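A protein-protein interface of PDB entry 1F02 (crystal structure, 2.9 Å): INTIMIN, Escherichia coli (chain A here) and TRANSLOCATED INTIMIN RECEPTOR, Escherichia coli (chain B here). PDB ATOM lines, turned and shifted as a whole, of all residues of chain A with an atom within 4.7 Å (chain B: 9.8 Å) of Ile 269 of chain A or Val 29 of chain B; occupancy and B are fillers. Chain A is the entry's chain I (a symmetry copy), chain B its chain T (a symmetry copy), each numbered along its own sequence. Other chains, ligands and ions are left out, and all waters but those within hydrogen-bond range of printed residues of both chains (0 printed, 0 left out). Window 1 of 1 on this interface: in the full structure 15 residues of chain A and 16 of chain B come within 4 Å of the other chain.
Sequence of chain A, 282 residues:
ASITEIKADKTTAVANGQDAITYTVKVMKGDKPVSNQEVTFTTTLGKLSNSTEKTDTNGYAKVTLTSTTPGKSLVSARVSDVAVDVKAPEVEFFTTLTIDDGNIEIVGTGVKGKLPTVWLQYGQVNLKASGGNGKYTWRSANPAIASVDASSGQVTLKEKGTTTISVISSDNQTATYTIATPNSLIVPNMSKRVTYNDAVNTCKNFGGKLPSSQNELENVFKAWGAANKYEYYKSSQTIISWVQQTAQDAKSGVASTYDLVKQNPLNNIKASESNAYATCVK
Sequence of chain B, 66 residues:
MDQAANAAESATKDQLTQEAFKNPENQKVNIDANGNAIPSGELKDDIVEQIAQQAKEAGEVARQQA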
ATOM      1  N   TRP A 242      22.281 -12.178  33.534  1.00  0.00           N
ATOM      2  CA  TRP A 242      22.128 -10.768  33.878  1.00  0.00           C
ATOM      3  C   TRP A 242      23.033 -10.430  35.040  1.00  0.00           C
ATOM      4  O   TRP A 242      23.140 -11.189  35.997  1.00  0.00           O
ATOM      5  CB  TRP A 242      20.681 -10.446  34.281  1.00  0.00           C
ATOM      6  CG  TRP A 242      19.722 -10.271  33.132  1.00  0.00           C
ATOM      7  CD1 TRP A 242      18.583 -10.997  32.892  1.00  0.00           C
ATOM      8  CD2 TRP A 242      19.826  -9.322  32.064  1.00  0.00           C
ATOM      9  NE1 TRP A 242      17.976 -10.557  31.738  1.00  0.00           N
ATOM     10  CE2 TRP A 242      18.716  -9.529  31.210  1.00  0.00           C
ATOM     11  CE3 TRP A 242      20.748  -8.319  31.743  1.00  0.00           C
ATOM     12  CZ2 TRP A 242      18.505  -8.767  30.051  1.00  0.00           C
ATOM     13  CZ3 TRP A 242      20.538  -7.560  30.587  1.00  0.00           C
ATOM     14  CH2 TRP A 242      19.424  -7.791  29.757  1.00  0.00           C
ATOM     15  N   GLY A 253      19.596   2.515  30.220  1.00  0.00           N
ATOM     16  CA  GLY A 253      18.610   1.463  30.050  1.00  0.00           C
ATOM     17  C   GLY A 253      19.216   0.149  29.587  1.00  0.00           C
ATOM     18  O   GLY A 253      18.601  -0.596  28.824  1.00  0.00           O
ATOM     19  N   VAL A 254      20.428  -0.143  30.045  1.00  0.00           N
ATOM     20  CA  VAL A 254      21.101  -1.382  29.666  1.00  0.00           C
ATOM     21  C   VAL A 254      21.826  -2.063  30.829  1.00  0.00           C
ATOM     22  O   VAL A 254      21.937  -1.507  31.927  1.00  0.00           O
ATOM     23  CB  VAL A 254      22.113  -1.136  28.531  1.00  0.00           C
ATOM     24  CG1 VAL A 254      21.380  -0.758  27.273  1.00  0.00           C
ATOM     25  CG2 VAL A 254      23.088  -0.039  28.920  1.00  0.00           C
ATOM     26  N   ALA A 255      22.315  -3.277  30.576  1.00  0.00           N
ATOM     27  CA  ALA A 255      23.033  -4.046  31.586  1.00  0.00           C
ATOM     28  C   ALA A 255      24.213  -4.787  30.968  1.00  0.00           C
ATOM     29  O   ALA A 255      24.498  -4.646  29.774  1.00  0.00           O
ATOM     30  CB  ALA A 255      22.089  -5.036  32.255  1.00  0.00           C
ATOM     31  N   THR A 257      26.402  -8.727  30.914  1.00  0.00           N
ATOM     32  CA  THR A 257      26.113 -10.150  31.056  1.00  0.00           C
ATOM     33  C   THR A 257      27.315 -11.060  30.946  1.00  0.00           C
ATOM     34  O   THR A 257      28.184 -10.860  30.097  1.00  0.00           O
ATOM     35  CB  THR A 257      25.118 -10.634  29.992  1.00  0.00           C
ATOM     36  OG1 THR A 257      25.624 -10.320  28.687  1.00  0.00           O
ATOM     37  CG2 THR A 257      23.765  -9.983  30.197  1.00  0.00           C
ATOM     38  N   LEU A 266      29.610  -9.420  28.028  1.00  0.00           N
ATOM     39  CA  LEU A 266      29.041  -8.406  27.137  1.00  0.00           C
ATOM     40  C   LEU A 266      28.498  -7.181  27.864  1.00  0.00           C
ATOM     41  O   LEU A 266      28.199  -7.235  29.060  1.00  0.00           O
ATOM     42  CB  LEU A 266      27.910  -9.019  26.304  1.00  0.00           C
ATOM     43  CG  LEU A 266      28.227 -10.206  25.393  1.00  0.00           C
ATOM     44  CD1 LEU A 266      26.960 -10.657  24.675  1.00  0.00           C
ATOM     45  CD2 LEU A 266      29.282  -9.814  24.390  1.00  0.00           C
ATOM     46  N   ASN A 267      28.353  -6.082  27.127  1.00  0.00           N
ATOM     47  CA  ASN A 267      27.837  -4.845  27.703  1.00  0.00           C
ATOM     48  C   ASN A 267      26.808  -4.132  26.836  1.00  0.00           C
ATOM     49  O   ASN A 267      26.597  -4.494  25.676  1.00  0.00           O
ATOM     50  CB  ASN A 267      28.991  -3.901  28.011  1.00  0.00           C
ATOM     51  CG  ASN A 267      29.854  -4.414  29.131  1.00  0.00           C
ATOM     52  OD1 ASN A 267      29.369  -4.635  30.241  1.00  0.00           O
ATOM     53  ND2 ASN A 267      31.135  -4.622  28.850  1.00  0.00           N
ATOM     54  N   ASN A 268      26.168  -3.119  27.415  1.00  0.00           N
ATOM     55  CA  ASN A 268      25.153  -2.343  26.714  1.00  0.00           C
ATOM     56  C   ASN A 268      24.118  -3.274  26.107  1.00  0.00           C
ATOM     57  O   ASN A 268      23.862  -3.235  24.905  1.00  0.00           O
ATOM     58  CB  ASN A 268      25.787  -1.503  25.602  1.00  0.00           C
ATOM     59  CG  ASN A 268      26.989  -0.717  26.078  1.00  0.00           C
ATOM     60  OD1 ASN A 268      26.959  -0.095  27.141  1.00  0.00           O
ATOM     61  ND2 ASN A 268      28.055  -0.728  25.283  1.00  0.00           N
ATOM     62  N   ILE A 269      23.532  -4.122  26.938  1.00  0.00           N
ATOM     63  CA  ILE A 269      22.525  -5.047  26.458  1.00  0.00           C
ATOM     64  C   ILE A 269      21.159  -4.462  26.792  1.00  0.00           C
ATOM     65  O   ILE A 269      21.014  -3.763  27.797  1.00  0.00           O
ATOM     66  CB  ILE A 269      22.677  -6.429  27.141  1.00  0.00           C
ATOM     67  CG1 ILE A 269      24.132  -6.891  27.039  1.00  0.00           C
ATOM     68  CG2 ILE A 269      21.757  -7.464  26.479  1.00  0.00           C
ATOM     69  CD1 ILE A 269      24.641  -7.021  25.623  1.00  0.00           C
ATOM     70  N   LYS A 270      20.167  -4.729  25.941  1.00  0.00           N
ATOM     71  CA  LYS A 270      18.806  -4.243  26.170  1.00  0.00           C
ATOM     72  C   LYS A 270      18.329  -4.684  27.540  1.00  0.00           C
ATOM     73  O   LYS A 270      18.084  -5.868  27.759  1.00  0.00           O
ATOM     74  CB  LYS A 270      17.840  -4.803  25.122  1.00  0.00           C
ATOM     75  CG  LYS A 270      17.943  -4.143  23.770  1.00  0.00           C
ATOM     76  CD  LYS A 270      17.786  -2.628  23.883  1.00  0.00           C
ATOM     77  CE  LYS A 270      16.464  -2.212  24.524  1.00  0.00           C
ATOM     78  NZ  LYS A 270      15.291  -2.683  23.744  1.00  0.00           N
ATOM     79  N   ALA A 271      18.195  -3.734  28.458  1.00  0.00           N
ATOM     80  CA  ALA A 271      17.751  -4.068  29.800  1.00  0.00           C
ATOM     81  C   ALA A 271      16.274  -4.478  29.799  1.00  0.00           C
ATOM     82  O   ALA A 271      15.803  -5.184  30.702  1.00  0.00           O
ATOM     83  CB  ALA A 271      17.977  -2.883  30.737  1.00  0.00           C
ATOM     84  N   ASN A 275      16.653 -10.656  26.887  1.00  0.00           N
ATOM     85  CA  ASN A 275      17.971 -11.049  26.373  1.00  0.00           C
ATOM     86  C   ASN A 275      18.786 -12.096  27.144  1.00  0.00           C
ATOM     87  O   ASN A 275      19.456 -12.929  26.531  1.00  0.00           O
ATOM     88  CB  ASN A 275      18.851  -9.806  26.184  1.00  0.00           C
ATOM     89  CG  ASN A 275      18.505  -9.028  24.930  1.00  0.00           C
ATOM     90  OD1 ASN A 275      18.375  -9.603  23.849  1.00  0.00           O
ATOM     91  ND2 ASN A 275      18.372  -7.716  25.065  1.00  0.00           N
ATOM     92  N   ASN B  23      29.161   5.932  16.695  1.00  0.00           N
ATOM     93  CA  ASN B  23      29.821   5.536  17.934  1.00  0.00           C
ATOM     94  C   ASN B  23      29.018   4.403  18.593  1.00  0.00           C
ATOM     95  O   ASN B  23      27.889   4.607  19.062  1.00  0.00           O
ATOM     96  CB  ASN B  23      29.912   6.725  18.887  1.00  0.00           C
ATOM     97  CG  ASN B  23      30.481   6.339  20.231  1.00  0.00           C
ATOM     98  OD1 ASN B  23      30.548   7.157  21.149  1.00  0.00           O
ATOM     99  ND2 ASN B  23      30.902   5.082  20.355  1.00  0.00           N
ATOM    100  N   PRO B  24      29.605   3.193  18.645  1.00  0.00           N
ATOM    101  CA  PRO B  24      29.001   1.986  19.225  1.00  0.00           C
ATOM    102  C   PRO B  24      28.564   2.160  20.668  1.00  0.00           C
ATOM    103  O   PRO B  24      27.548   1.616  21.085  1.00  0.00           O
ATOM    104  CB  PRO B  24      30.108   0.951  19.086  1.00  0.00           C
ATOM    105  CG  PRO B  24      30.850   1.414  17.877  1.00  0.00           C
ATOM    106  CD  PRO B  24      30.948   2.892  18.127  1.00  0.00           C
ATOM    107  N   GLU B  25      29.351   2.918  21.422  1.00  0.00           N
ATOM    108  CA  GLU B  25      29.074   3.193  22.831  1.00  0.00           C
ATOM    109  C   GLU B  25      27.591   3.450  23.094  1.00  0.00           C
ATOM    110  O   GLU B  25      26.933   2.741  23.865  1.00  0.00           O
ATOM    111  CB  GLU B  25      29.865   4.429  23.273  1.00  0.00           C
ATOM    112  CG  GLU B  25      31.368   4.323  23.096  1.00  0.00           C
ATOM    113  CD  GLU B  25      32.023   3.503  24.185  1.00  0.00           C
ATOM    114  OE1 GLU B  25      31.516   2.398  24.488  1.00  0.00           O
ATOM    115  OE2 GLU B  25      33.050   3.968  24.732  1.00  0.00           O
ATOM    116  N   ASN B  26      27.092   4.488  22.432  1.00  0.00           N
ATOM    117  CA  ASN B  26      25.716   4.950  22.546  1.00  0.00           C
ATOM    118  C   ASN B  26      24.657   3.917  22.198  1.00  0.00           C
ATOM    119  O   ASN B  26      23.518   4.020  22.653  1.00  0.00           O
ATOM    120  CB  ASN B  26      25.535   6.163  21.641  1.00  0.00           C
ATOM    121  CG  ASN B  26      26.720   7.103  21.688  1.00  0.00           C
ATOM    122  OD1 ASN B  26      26.979   7.844  20.737  1.00  0.00           O
ATOM    123  ND2 ASN B  26      27.446   7.086  22.802  1.00  0.00           N
ATOM    124  N   GLN B  27      25.018   2.927  21.393  1.00  0.00           N
ATOM    125  CA  GLN B  27      24.049   1.922  20.979  1.00  0.00           C
ATOM    126  C   GLN B  27      23.708   0.872  22.015  1.00  0.00           C
ATOM    127  O   GLN B  27      24.333   0.779  23.070  1.00  0.00           O
ATOM    128  CB  GLN B  27      24.531   1.222  19.721  1.00  0.00           C
ATOM    129  CG  GLN B  27      25.062   2.175  18.694  1.00  0.00           C
ATOM    130  CD  GLN B  27      25.161   1.540  17.337  1.00  0.00           C
ATOM    131  OE1 GLN B  27      25.777   2.098  16.433  1.00  0.00           O
ATOM    132  NE2 GLN B  27      24.544   0.366  17.178  1.00  0.00           N
ATOM    133  N   LYS B  28      22.687   0.091  21.695  1.00  0.00           N
ATOM    134  CA  LYS B  28      22.232  -0.988  22.553  1.00  0.00           C
ATOM    135  C   LYS B  28      22.544  -2.273  21.803  1.00  0.00           C
ATOM    136  O   LYS B  28      22.917  -2.233  20.622  1.00  0.00           O
ATOM    137  CB  LYS B  28      20.724  -0.889  22.797  1.00  0.00           C
ATOM    138  CG  LYS B  28      20.286   0.243  23.712  1.00  0.00           C
ATOM    139  CD  LYS B  28      18.772   0.187  23.920  1.00  0.00           C
ATOM    140  CE  LYS B  28      18.274   1.134  25.010  1.00  0.00           C
ATOM    141  NZ  LYS B  28      16.809   0.964  25.260  1.00  0.00           N
ATOM    142  N   VAL B  29      22.386  -3.408  22.476  1.00  0.00           N
ATOM    143  CA  VAL B  29      22.657  -4.700  21.857  1.00  0.00           C
ATOM    144  C   VAL B  29      21.685  -5.774  22.341  1.00  0.00           C
ATOM    145  O   VAL B  29      21.167  -5.701  23.460  1.00  0.00           O
ATOM    146  CB  VAL B  29      24.108  -5.158  22.162  1.00  0.00           C
ATOM    147  CG1 VAL B  29      24.416  -6.482  21.461  1.00  0.00           C
ATOM    148  CG2 VAL B  29      25.084  -4.086  21.722  1.00  0.00           C
ATOM    149  N   ASN B  30      21.438  -6.761  21.481  1.00  0.00           N
ATOM    150  CA  ASN B  30      20.555  -7.873  21.802  1.00  0.00           C
ATOM    151  C   ASN B  30      21.264  -9.212  21.735  1.00  0.00           C
ATOM    152  O   ASN B  30      22.416  -9.304  21.308  1.00  0.00           O
ATOM    153  CB  ASN B  30      19.350  -7.885  20.875  1.00  0.00           C
ATOM    154  CG  ASN B  30      18.330  -6.860  21.271  1.00  0.00           C
ATOM    155  OD1 ASN B  30      17.873  -6.846  22.416  1.00  0.00           O
ATOM    156  ND2 ASN B  30      17.968  -5.986  20.340  1.00  0.00           N
ATOM    157  N   ILE B  31      20.562 -10.257  22.152  1.00  0.00           N
ATOM    158  CA  ILE B  31      21.138 -11.590  22.177  1.00  0.00           C
ATOM    159  C   ILE B  31      20.401 -12.567  21.268  1.00  0.00           C
ATOM    160  O   ILE B  31      19.230 -12.873  21.510  1.00  0.00           O
ATOM    161  CB  ILE B  31      21.097 -12.176  23.613  1.00  0.00           C
ATOM    162  CG1 ILE B  31      21.699 -11.194  24.630  1.00  0.00           C
ATOM    163  CG2 ILE B  31      21.843 -13.486  23.638  1.00  0.00           C
ATOM    164  CD1 ILE B  31      23.202 -10.953  24.484  1.00  0.00           C
ATOM    165  N   ASP B  32      21.067 -13.064  20.229  1.00  0.00           N
ATOM    166  CA  ASP B  32      20.408 -14.032  19.358  1.00  0.00           C
ATOM    167  C   ASP B  32      20.309 -15.308  20.167  1.00  0.00           C
ATOM    168  O   ASP B  32      21.041 -15.470  21.140  1.00  0.00           O
ATOM    169  CB  ASP B  32      21.209 -14.291  18.082  1.00  0.00           C
ATOM    170  CG  ASP B  32      22.618 -14.755  18.362  1.00  0.00           C
ATOM    171  OD1 ASP B  32      22.805 -15.688  19.177  1.00  0.00           O
ATOM    172  OD2 ASP B  32      23.544 -14.185  17.748  1.00  0.00           O
ATOM    173  N   GLY B  35      22.842 -16.959  22.137  1.00  0.00           N
ATOM    174  CA  GLY B  35      23.402 -16.200  23.239  1.00  0.00           C
ATOM    175  C   GLY B  35      24.492 -15.240  22.797  1.00  0.00           C
ATOM    176  O   GLY B  35      25.303 -14.766  23.606  1.00  0.00           O
ATOM    177  N   ASN B  36      24.523 -14.946  21.504  1.00  0.00           N
ATOM    178  CA  ASN B  36      25.528 -14.035  20.986  1.00  0.00           C
ATOM    179  C   ASN B  36      24.960 -12.636  20.768  1.00  0.00           C
ATOM    180  O   ASN B  36      23.756 -12.460  20.529  1.00  0.00           O
ATOM    181  CB  ASN B  36      26.108 -14.583  19.686  1.00  0.00           C
ATOM    182  CG  ASN B  36      26.734 -15.944  19.865  1.00  0.00           C
ATOM    183  OD1 ASN B  36      27.634 -16.126  20.690  1.00  0.00           O
ATOM    184  ND2 ASN B  36      26.262 -16.915  19.093  1.00  0.00           N
ATOM    185  N   ALA B  37      25.834 -11.641  20.860  1.00  0.00           N
ATOM    186  CA  ALA B  37      25.430 -10.255  20.691  1.00  0.00           C
ATOM    187  C   ALA B  37      25.022  -9.963  19.264  1.00  0.00           C
ATOM    188  O   ALA B  37      25.470 -10.632  18.331  1.00  0.00           O
ATOM    189  CB  ALA B  37      26.558  -9.330  21.095  1.00  0.00           C
ATOM    190  N   ILE B  38      24.165  -8.955  19.115  1.00  0.00           N
ATOM    191  CA  ILE B  38      23.668  -8.504  17.816  1.00  0.00           C
ATOM    192  C   ILE B  38      23.312  -7.021  17.886  1.00  0.00           C
ATOM    193  O   ILE B  38      22.950  -6.501  18.943  1.00  0.00           O
ATOM    194  CB  ILE B  38      22.412  -9.291  17.370  1.00  0.00           C
ATOM    195  CG1 ILE B  38      21.450  -9.449  18.548  1.00  0.00           C
ATOM    196  CG2 ILE B  38      22.818 -10.630  16.785  1.00  0.00           C
ATOM    197  CD1 ILE B  38      20.173 -10.160  18.202  1.00  0.00           C
ATOM    198  N   PRO B  39      23.420  -6.316  16.752  1.00  0.00           N
ATOM    199  CA  PRO B  39      23.097  -4.889  16.734  1.00  0.00           C
ATOM    200  C   PRO B  39      21.589  -4.662  16.661  1.00  0.00           C
ATOM    201  O   PRO B  39      20.887  -5.361  15.931  1.00  0.00           O
ATOM    202  CB  PRO B  39      23.814  -4.403  15.480  1.00  0.00           C
ATOM    203  CG  PRO B  39      23.617  -5.562  14.545  1.00  0.00           C
ATOM    204  CD  PRO B  39      23.917  -6.760  15.434  1.00  0.00           C
ATOM    205  N   SER B  40      21.093  -3.704  17.435  1.00  0.00           N
ATOM    206  CA  SER B  40      19.670  -3.371  17.418  1.00  0.00           C
ATOM    207  C   SER B  40      19.545  -1.855  17.336  1.00  0.00           C
ATOM    208  O   SER B  40      19.649  -1.168  18.354  1.00  0.00           O
ATOM    209  CB  SER B  40      18.965  -3.886  18.677  1.00  0.00           C
ATOM    210  OG  SER B  40      17.551  -3.811  18.533  1.00  0.00           O
ATOM    211  N   GLY B  41      19.338  -1.363  16.113  1.00  0.00           N
ATOM    212  CA  GLY B  41      19.216   0.062  15.828  1.00  0.00           C
ATOM    213  C   GLY B  41      19.006   1.044  16.966  1.00  0.00           C
ATOM    214  O   GLY B  41      19.531   2.157  16.946  1.00  0.00           O
ATOM    215  N   GLU B  42      18.231   0.635  17.961  1.00  0.00           N
ATOM    216  CA  GLU B  42      17.939   1.479  19.111  1.00  0.00           C
ATOM    217  C   GLU B  42      19.183   2.012  19.832  1.00  0.00           C
ATOM    218  O   GLU B  42      20.186   1.304  19.975  1.00  0.00           O
ATOM    219  CB  GLU B  42      17.068   0.689  20.080  1.00  0.00           C
ATOM    220  CG  GLU B  42      15.927  -0.026  19.376  1.00  0.00           C
ATOM    221  CD  GLU B  42      15.106  -0.870  20.317  1.00  0.00           C
ATOM    222  OE1 GLU B  42      14.669  -0.333  21.358  1.00  0.00           O
ATOM    223  OE2 GLU B  42      14.893  -2.066  20.013  1.00  0.00           O
ATOM    224  N   LEU B  43      19.109   3.269  20.273  1.00  0.00           N
ATOM    225  CA  LEU B  43      20.201   3.906  21.005  1.00  0.00           C
ATOM    226  C   LEU B  43      19.883   3.868  22.501  1.00  0.00           C
ATOM    227  O   LEU B  43      18.740   3.610  22.886  1.00  0.00           O
ATOM    228  CB  LEU B  43      20.353   5.369  20.581  1.00  0.00           C
ATOM    229  CG  LEU B  43      20.827   5.740  19.177  1.00  0.00           C
ATOM    230  CD1 LEU B  43      20.818   7.249  19.045  1.00  0.00           C
ATOM    231  CD2 LEU B  43      22.233   5.219  18.929  1.00  0.00           C
ATOM    232  N   LYS B  44      20.889   4.127  23.339  1.00  0.00           N
ATOM    233  CA  LYS B  44      20.698   4.150  24.796  1.00  0.00           C
ATOM    234  C   LYS B  44      19.716   5.262  25.181  1.00  0.00           C
ATOM    235  O   LYS B  44      19.771   6.373  24.634  1.00  0.00           O
ATOM    236  CB  LYS B  44      22.022   4.403  25.527  1.00  0.00           C
ATOM    237  CG  LYS B  44      22.965   3.220  25.637  1.00  0.00           C
ATOM    238  CD  LYS B  44      24.228   3.665  26.347  1.00  0.00           C
ATOM    239  CE  LYS B  44      25.289   2.597  26.345  1.00  0.00           C
ATOM    240  NZ  LYS B  44      26.613   3.202  26.676  1.00  0.00           N
ATOM    241  N   ASP B  45      18.842   4.967  26.142  1.00  0.00           N
ATOM    242  CA  ASP B  45      17.836   5.920  26.593  1.00  0.00           C
ATOM    243  C   ASP B  45      18.380   7.296  26.972  1.00  0.00           C
ATOM    244  O   ASP B  45      17.863   8.313  26.507  1.00  0.00           O
ATOM    245  CB  ASP B  45      17.054   5.320  27.753  1.00  0.00           C
ATOM    246  CG  ASP B  45      16.524   3.941  27.430  1.00  0.00           C
ATOM    247  OD1 ASP B  45      16.181   3.706  26.254  1.00  0.00           O
ATOM    248  OD2 ASP B  45      16.441   3.091  28.344  1.00  0.00           O
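Printed residues of chain B within 4 Å of Gly 253 of chain A: Asp 45 (3.2 Å). Of chain B, only Glu 25 (3.9 Å), Gln 27 (3.7 Å), Lys 28 (3.5 Å), Val 29 (2.8 Å) and Lys 44 (3.3 Å) come within 4 Å of Asn 268 of chain A. Ile 269 of chain A touches just one residue of chain B: Val 29 (3.4 Å). Printed residues of chain B within 4 Å of Asn 275 of chain A: Val 29, Asn 30 and Ile 31. Pro 24 of chain B touches none of the printed residues of chain A. Printed residues of chain A within 4 Å of Lys 28 of chain B: Val 254, Asn 268 and Lys 270. Of chain A, only Asn 268 (2.8 Å), Ile 269 (3.4 Å), Lys 270 (2.8 Å) and Asn 275 (3.8 Å) come within 4 Å of Val 29 of chain B. Printed residues of chain A within 4 Å of Ala 37 of chain B: Leu 266. Of the printed residues of chain A, Lys 44 of chain B touches Asn 268 (3.3 Å). The nearest residue of chain A that does not touch Val 29 of chain B is Asn 267 of chain A (4.3 Å). The nearest printed residue of chain A that does not touch Glu 42 of chain B is Asn 268 of chain A (7.6 Å).
The backbone carbonyl oxygen (O) of Thr 257 of chain A sits at hydrogen-bond distance from the backbone NH (N) of Leu 266 of chain A (2.9 Å). O of Asn 26 of chain B is in hydrogen-bond range of N of Lys 44 of chain B (2.7 Å). ND2 of Asn 23 of chain B lies close to N of Glu 25 of chain B (2.9 Å). O of Gly 253 of chain A lies close to N of Ala 271 of chain A (3.2 Å). The backbone carbonyl oxygen (O) of Glu 42 of chain B lies within hydrogen-bond range of the backbone NH (N) of Lys 28 of chain B (3.3 Å). OG of Ser 40 of chain B lies close to ND2 of Asn 30 of chain B.
Among the printed residues, pairs that only touch across the chains: Gly 253 of chain A with Asp 45 of chain B (3.2 Å), Val 254 of chain A with Lys 28 of chain B (3.9 Å), Leu 266 of chain A with Ile 31 of chain B (3.8 Å), Leu 266 of chain A with Ala 37 of chain B (3.8 Å), Asn 268 of chain A with Glu 25 of chain B (3.9 Å), Asn 268 of chain A with Gln 27 of chain B (3.7 Å), Asn 268 of chain A with Lys 28 of chain B (3.5 Å), Ile 269 of chain A with Val 29 of chain B (3.4 Å), Lys 270 of chain A with Lys 28 of chain B (3.0 Å), Lys 270 of chain A with Asn 30 of chain B (3.0 Å) and Asn 275 of chain A with Val 29 of chain B (3.8 Å).
Along chain B the printed residues that touch a printed residue of chain A span positions 25 to 45. Of the 12 printed residues of chain A, 7 touch a printed residue of chain B. Among the printed residues, Asp or Glu carboxylates within 4 Å of a Lys or Arg side-chain nitrogen of the other chain: Lys 270 of chain A with Glu 42 of chain B.
The backbone NH (N) of Val 29 of chain B sits at hydrogen-bond distance from the backbone carbonyl oxygen (O) of Asn 268 of chain A (2.8 Å). The side-chain amide nitrogen (ND2) of Asn 275 of chain A is in hydrogen-bond range of the side-chain amide oxygen (OD1) of Asn 30 of chain B, 2.8 Å away. N of Lys 270 of chain A sits at hydrogen-bond distance from O of Val 29 of chain B (2.8 Å). The backbone NH (N) of Ile 31 of chain B lies within hydrogen-bond range of the side-chain amide oxygen (OD1) of Asn 275 of chain A (2.8 Å). OD1 of Asn 268 of chain A lies close to NZ of Lys 44 of chain B (3.3 Å). The side-chain carboxylate of Glu 42 of chain B lies within salt-bridge range of the side-chain amino group of Lys 270 of chain A (3.4 Å).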
